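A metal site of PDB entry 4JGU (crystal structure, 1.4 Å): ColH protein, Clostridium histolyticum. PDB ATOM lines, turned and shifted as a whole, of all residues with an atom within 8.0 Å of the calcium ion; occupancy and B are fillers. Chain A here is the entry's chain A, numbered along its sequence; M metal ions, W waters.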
ATOM      1  N   LEU A   6      -3.524 -22.592  -1.400  1.00  0.00           N
ATOM      2  CA  LEU A   6      -3.948 -23.694  -0.543  1.00  0.00           C
ATOM      3  C   LEU A   6      -4.394 -23.253   0.838  1.00  0.00           C
ATOM      4  O   LEU A   6      -5.208 -23.954   1.482  1.00  0.00           O
ATOM      5  CB  LEU A   6      -2.787 -24.669  -0.371  1.00  0.00           C
ATOM      6  CG  LEU A   6      -2.624 -25.559  -1.619  1.00  0.00           C
ATOM      7  CD1 LEU A   6      -1.149 -26.186  -1.625  1.00  0.00           C
ATOM      8  CD2 LEU A   6      -3.675 -26.709  -1.597  1.00  0.00           C
ATOM      9  N   GLU A   8      -6.388 -21.032   1.569  1.00  0.00           N
ATOM     10  CA  GLU A   8      -7.828 -20.686   1.508  1.00  0.00           C
ATOM     11  C   GLU A   8      -8.707 -21.927   1.527  1.00  0.00           C
ATOM     12  O   GLU A   8      -9.964 -21.803   1.576  1.00  0.00           O
ATOM     13  CB  GLU A   8      -8.123 -19.913   0.180  1.00  0.00           C
ATOM     14  CG  GLU A   8      -7.319 -18.631   0.055  1.00  0.00           C
ATOM     15  CD  GLU A   8      -7.816 -17.677  -1.022  1.00  0.00           C
ATOM     16  OE1 GLU A   8      -8.845 -17.913  -1.715  1.00  0.00           O
ATOM     17  OE2 GLU A   8      -7.124 -16.620  -1.159  1.00  0.00           O
ATOM     18  N   ASN A   9      -8.114 -23.130   1.502  1.00  0.00           N
ATOM     19  CA  ASN A   9      -8.924 -24.363   1.460  1.00  0.00           C
ATOM     20  C   ASN A   9      -9.765 -24.507   2.699  1.00  0.00           C
ATOM     21  O   ASN A   9      -9.255 -24.380   3.816  1.00  0.00           O
ATOM     22  CB  ASN A   9      -7.963 -25.594   1.380  1.00  0.00           C
ATOM     23  CG  ASN A   9      -8.717 -26.875   1.458  1.00  0.00           C
ATOM     24  OD1 ASN A   9      -9.645 -27.095   0.679  1.00  0.00           O
ATOM     25  ND2 ASN A   9      -8.344 -27.754   2.402  1.00  0.00           N
ATOM     26  N   LYS A  10     -11.032 -24.848   2.504  1.00  0.00           N
ATOM     27  CA  LYS A  10     -11.905 -25.240   3.631  1.00  0.00           C
ATOM     28  C   LYS A  10     -11.696 -26.700   3.987  1.00  0.00           C
ATOM     29  O   LYS A  10     -11.633 -27.571   3.115  1.00  0.00           O
ATOM     30  CB  LYS A  10     -13.383 -25.001   3.282  1.00  0.00           C
ATOM     31  CG  LYS A  10     -13.657 -23.546   3.016  1.00  0.00           C
ATOM     32  CD  LYS A  10     -15.064 -23.313   2.608  1.00  0.00           C
ATOM     33  CE  LYS A  10     -15.301 -21.796   2.594  1.00  0.00           C
ATOM     34  NZ  LYS A  10     -16.689 -21.353   2.446  1.00  0.00           N
ATOM     35  N   LEU A  11     -11.567 -26.955   5.293  1.00  0.00           N
ATOM     36  CA  LEU A  11     -11.288 -28.305   5.760  1.00  0.00           C
ATOM     37  C   LEU A  11     -12.567 -29.178   5.692  1.00  0.00           C
ATOM     38  O   LEU A  11     -13.705 -28.684   5.769  1.00  0.00           O
ATOM     39  CB  LEU A  11     -10.767 -28.291   7.201  1.00  0.00           C
ATOM     40  CG  LEU A  11      -9.446 -27.545   7.399  1.00  0.00           C
ATOM     41  CD1 LEU A  11      -9.170 -27.339   8.842  1.00  0.00           C
ATOM     42  CD2 LEU A  11      -8.353 -28.180   6.602  1.00  0.00           C
ATOM     43  N   PRO A  12     -12.374 -30.485   5.710  1.00  0.00           N
ATOM     44  CA  PRO A  12     -13.520 -31.374   5.717  1.00  0.00           C
ATOM     45  C   PRO A  12     -14.286 -31.295   7.055  1.00  0.00           C
ATOM     46  O   PRO A  12     -13.684 -31.042   8.137  1.00  0.00           O
ATOM     47  CB  PRO A  12     -12.882 -32.762   5.492  1.00  0.00           C
ATOM     48  CG  PRO A  12     -11.503 -32.650   5.788  1.00  0.00           C
ATOM     49  CD  PRO A  12     -11.099 -31.234   5.590  1.00  0.00           C
ATOM     50  N   VAL A  13     -15.602 -31.419   6.945  1.00  0.00           N
ATOM     51  CA  VAL A  13     -16.495 -31.434   8.087  1.00  0.00           C
ATOM     52  C   VAL A  13     -16.928 -32.874   8.372  1.00  0.00           C
ATOM     53  O   VAL A  13     -17.554 -33.522   7.516  1.00  0.00           O
ATOM     54  CB  VAL A  13     -17.768 -30.525   7.845  1.00  0.00           C
ATOM     55  CG1 VAL A  13     -18.706 -30.580   9.057  1.00  0.00           C
ATOM     56  CG2 VAL A  13     -17.311 -29.101   7.518  1.00  0.00           C
ATOM     57  N   TYR A  36     -18.267 -34.328   4.691  1.00  0.00           N
ATOM     58  CA  TYR A  36     -18.214 -33.580   3.381  1.00  0.00           C
ATOM     59  C   TYR A  36     -17.154 -32.545   3.411  1.00  0.00           C
ATOM     60  O   TYR A  36     -16.740 -32.096   4.486  1.00  0.00           O
ATOM     61  CB  TYR A  36     -19.603 -32.942   3.020  1.00  0.00           C
ATOM     62  CG  TYR A  36     -19.938 -31.704   3.798  1.00  0.00           C
ATOM     63  CD1 TYR A  36     -20.361 -31.748   5.165  1.00  0.00           C
ATOM     64  CD2 TYR A  36     -19.816 -30.445   3.177  1.00  0.00           C
ATOM     65  CE1 TYR A  36     -20.652 -30.533   5.889  1.00  0.00           C
ATOM     66  CE2 TYR A  36     -20.103 -29.286   3.896  1.00  0.00           C
ATOM     67  CZ  TYR A  36     -20.511 -29.373   5.245  1.00  0.00           C
ATOM     68  OH  TYR A  36     -20.784 -28.230   5.944  1.00  0.00           O
ATOM     69  N   ASP A  37     -16.760 -32.126   2.201  1.00  0.00           N
ATOM     70  CA  ASP A  37     -15.804 -31.067   2.060  1.00  0.00           C
ATOM     71  C   ASP A  37     -16.534 -29.855   1.463  1.00  0.00           C
ATOM     72  O   ASP A  37     -16.960 -29.928   0.309  1.00  0.00           O
ATOM     73  CB  ASP A  37     -14.672 -31.492   1.094  1.00  0.00           C
ATOM     74  CG  ASP A  37     -13.582 -30.399   0.962  1.00  0.00           C
ATOM     75  OD1 ASP A  37     -13.720 -29.359   1.644  1.00  0.00           O
ATOM     76  OD2 ASP A  37     -12.653 -30.560   0.128  1.00  0.00           O
ATOM     77  N   PRO A  38     -16.667 -28.750   2.228  1.00  0.00           N
ATOM     78  CA  PRO A  38     -17.500 -27.618   1.724  1.00  0.00           C
ATOM     79  C   PRO A  38     -17.057 -27.117   0.348  1.00  0.00           C
ATOM     80  O   PRO A  38     -17.877 -26.561  -0.393  1.00  0.00           O
ATOM     81  CB  PRO A  38     -17.300 -26.539   2.804  1.00  0.00           C
ATOM     82  CG  PRO A  38     -16.963 -27.305   4.075  1.00  0.00           C
ATOM     83  CD  PRO A  38     -16.148 -28.471   3.602  1.00  0.00           C
ATOM     84  N   ASP A  39     -15.771 -27.176   0.035  1.00  0.00           N
ATOM     85  CA  ASP A  39     -15.302 -26.665  -1.255  1.00  0.00           C
ATOM     86  C   ASP A  39     -14.569 -27.693  -2.086  1.00  0.00           C
ATOM     87  O   ASP A  39     -13.812 -27.385  -3.007  1.00  0.00           O
ATOM     88  CB  ASP A  39     -14.434 -25.418  -1.039  1.00  0.00           C
ATOM     89  CG  ASP A  39     -13.109 -25.749  -0.296  1.00  0.00           C
ATOM     90  OD1 ASP A  39     -12.851 -26.977  -0.021  1.00  0.00           O
ATOM     91  OD2 ASP A  39     -12.358 -24.784  -0.006  1.00  0.00           O
ATOM     92  N   GLY A  40     -14.934 -28.968  -1.938  1.00  0.00           N
ATOM     93  CA  GLY A  40     -14.244 -30.035  -2.689  1.00  0.00           C
ATOM     94  C   GLY A  40     -14.901 -31.365  -2.457  1.00  0.00           C
ATOM     95  O   GLY A  40     -16.137 -31.490  -2.506  1.00  0.00           O
ATOM     96  N   SER A  41     -14.071 -32.364  -2.209  1.00  0.00           N
ATOM     97  CA  SER A  41     -14.610 -33.680  -1.943  1.00  0.00           C
ATOM     98  C   SER A  41     -13.750 -34.360  -0.880  1.00  0.00           C
ATOM     99  O   SER A  41     -12.607 -33.967  -0.623  1.00  0.00           O
ATOM    100  CB  SER A  41     -14.623 -34.559  -3.220  1.00  0.00           C
ATOM    101  OG  SER A  41     -15.177 -34.024  -4.378  1.00  0.00           O
ATOM    102  N   ILE A  42     -14.290 -35.444  -0.334  1.00  0.00           N
ATOM    103  CA  ILE A  42     -13.570 -36.253   0.628  1.00  0.00           C
ATOM    104  C   ILE A  42     -12.683 -37.228  -0.097  1.00  0.00           C
ATOM    105  O   ILE A  42     -13.090 -37.860  -1.074  1.00  0.00           O
ATOM    106  CB  ILE A  42     -14.556 -37.004   1.604  1.00  0.00           C
ATOM    107  CG1 ILE A  42     -15.391 -35.970   2.377  1.00  0.00           C
ATOM    108  CG2 ILE A  42     -13.788 -37.925   2.541  1.00  0.00           C
ATOM    109  CD1 ILE A  42     -14.587 -34.971   3.224  1.00  0.00           C
ATOM    110  N   MET A  78      -9.366 -36.790   5.296  1.00  0.00           N
ATOM    111  CA  MET A  78      -8.580 -35.953   4.368  1.00  0.00           C
ATOM    112  C   MET A  78      -9.483 -35.491   3.232  1.00  0.00           C
ATOM    113  O   MET A  78     -10.294 -36.298   2.700  1.00  0.00           O
ATOM    114  CB  MET A  78      -7.375 -36.766   3.859  1.00  0.00           C
ATOM    115  CG  MET A  78      -6.520 -36.064   2.936  1.00  0.00           C
ATOM    116  SD  MET A  78      -5.085 -37.066   2.385  1.00  0.00           S
ATOM    117  CE  MET A  78      -5.877 -38.586   1.995  1.00  0.00           C
ATOM    118  N   ASP A  79      -9.321 -34.240   2.788  1.00  0.00           N
ATOM    119  CA  ASP A  79     -10.077 -33.757   1.641  1.00  0.00           C
ATOM    120  C   ASP A  79      -9.265 -33.785   0.352  1.00  0.00           C
ATOM    121  O   ASP A  79      -8.114 -34.300   0.347  1.00  0.00           O
ATOM    122  CB  ASP A  79     -10.640 -32.330   1.913  1.00  0.00           C
ATOM    123  CG  ASP A  79      -9.596 -31.221   1.917  1.00  0.00           C
ATOM    124  OD1 ASP A  79      -8.419 -31.491   1.680  1.00  0.00           O
ATOM    125  OD2 ASP A  79     -10.017 -30.044   2.195  1.00  0.00           O
ATOM    126  N   SER A  80      -9.842 -33.221  -0.705  1.00  0.00           N
ATOM    127  CA  SER A  80      -9.242 -33.265  -2.035  1.00  0.00           C
ATOM    128  C   SER A  80      -8.060 -32.278  -2.189  1.00  0.00           C
ATOM    129  O   SER A  80      -7.478 -32.201  -3.266  1.00  0.00           O
ATOM    130  CB  SER A  80     -10.340 -33.023  -3.052  1.00  0.00           C
ATOM    131  OG  SER A  80     -10.936 -31.760  -2.750  1.00  0.00           O
ATOM    132  N   SER A  81      -7.694 -31.528  -1.127  1.00  0.00           N
ATOM    133  CA  SER A  81      -6.506 -30.731  -1.090  1.00  0.00           C
ATOM    134  C   SER A  81      -5.463 -31.312  -0.142  1.00  0.00           C
ATOM    135  O   SER A  81      -4.433 -30.621   0.139  1.00  0.00           O
ATOM    136  CB  SER A  81      -6.819 -29.262  -0.693  1.00  0.00           C
ATOM    137  OG  SER A  81      -7.710 -28.670  -1.672  1.00  0.00           O
ATOM    138  N   GLY A  82      -5.682 -32.542   0.357  1.00  0.00           N
ATOM    139  CA  GLY A  82      -4.715 -33.163   1.248  1.00  0.00           C
ATOM    140  C   GLY A  82      -4.708 -32.656   2.675  1.00  0.00           C
ATOM    141  O   GLY A  82      -3.799 -32.967   3.430  1.00  0.00           O
ATOM    142  N   GLN A  83      -5.745 -31.888   3.075  1.00  0.00           N
ATOM    143  CA  GLN A  83      -5.833 -31.300   4.385  1.00  0.00           C
ATOM    144  C   GLN A  83      -6.825 -32.082   5.253  1.00  0.00           C
ATOM    145  O   GLN A  83      -7.789 -32.746   4.737  1.00  0.00           O
ATOM    146  CB  GLN A  83      -6.152 -29.830   4.326  1.00  0.00           C
ATOM    147  CG  GLN A  83      -4.959 -29.050   3.615  1.00  0.00           C
ATOM    148  CD  GLN A  83      -5.188 -27.550   3.491  1.00  0.00           C
ATOM    149  OE1 GLN A  83      -6.114 -27.014   4.043  1.00  0.00           O
ATOM    150  NE2 GLN A  83      -4.275 -26.852   2.783  1.00  0.00           N
HETATM  151 CA    CA M   1     -11.514 -28.590   0.954  1.00  0.00          CA
HETATM  152  O   HOH W   1     -10.332 -29.399  -1.063  1.00  0.00           O
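OD1 of Asn 9 lies close to OG of Ser 81 (3.4 Å).
The side-chain amide oxygen (OE1) of Gln 83 is in hydrogen-bond range of the side-chain amide nitrogen (ND2) of Asn 9 (2.9 Å).
OD2 of Asp 37 sits close to N of Gly 40 (3.5 Å).
The side-chain carboxylate (OD2) of Asp 37 lies close to the backbone NH (N) of Ser 41, 3.3 Å away.
The side-chain carboxylate (OD1) of Asp 79 lies within hydrogen-bond range of the backbone NH (N) of Ser 81 (2.9 Å).
The side-chain carboxylate (OD1) of Asp 79 lies within hydrogen-bond range of the backbone NH (N) of Gln 83.
The side-chain carboxylate (OD1) of Asp 79 sits at hydrogen-bond distance from the backbone NH (N) of Gly 82, at 3.2 Å.
Water W1 bridges OG of Ser 81 and OG of Ser 80.
Within 4 Å of the calcium ion: Asn 9, Lys 10, Asp 37, Asp 39 and Asp 79.
The nearest printed residue that does not touch the calcium ion is Gly 40 (4.5 Å).
The calcium ion is bound by OD1 of Asp 39 (2.3 Å), O of Lys 10 (2.4 Å), OD1 of Asn 9 (2.4 Å), OD2 of Asp 37 (2.4 Å), OD2 of Asp 79 (2.4 Å), OD1 of Asp 37 (2.4 Å) and water W1 (2.5 Å).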
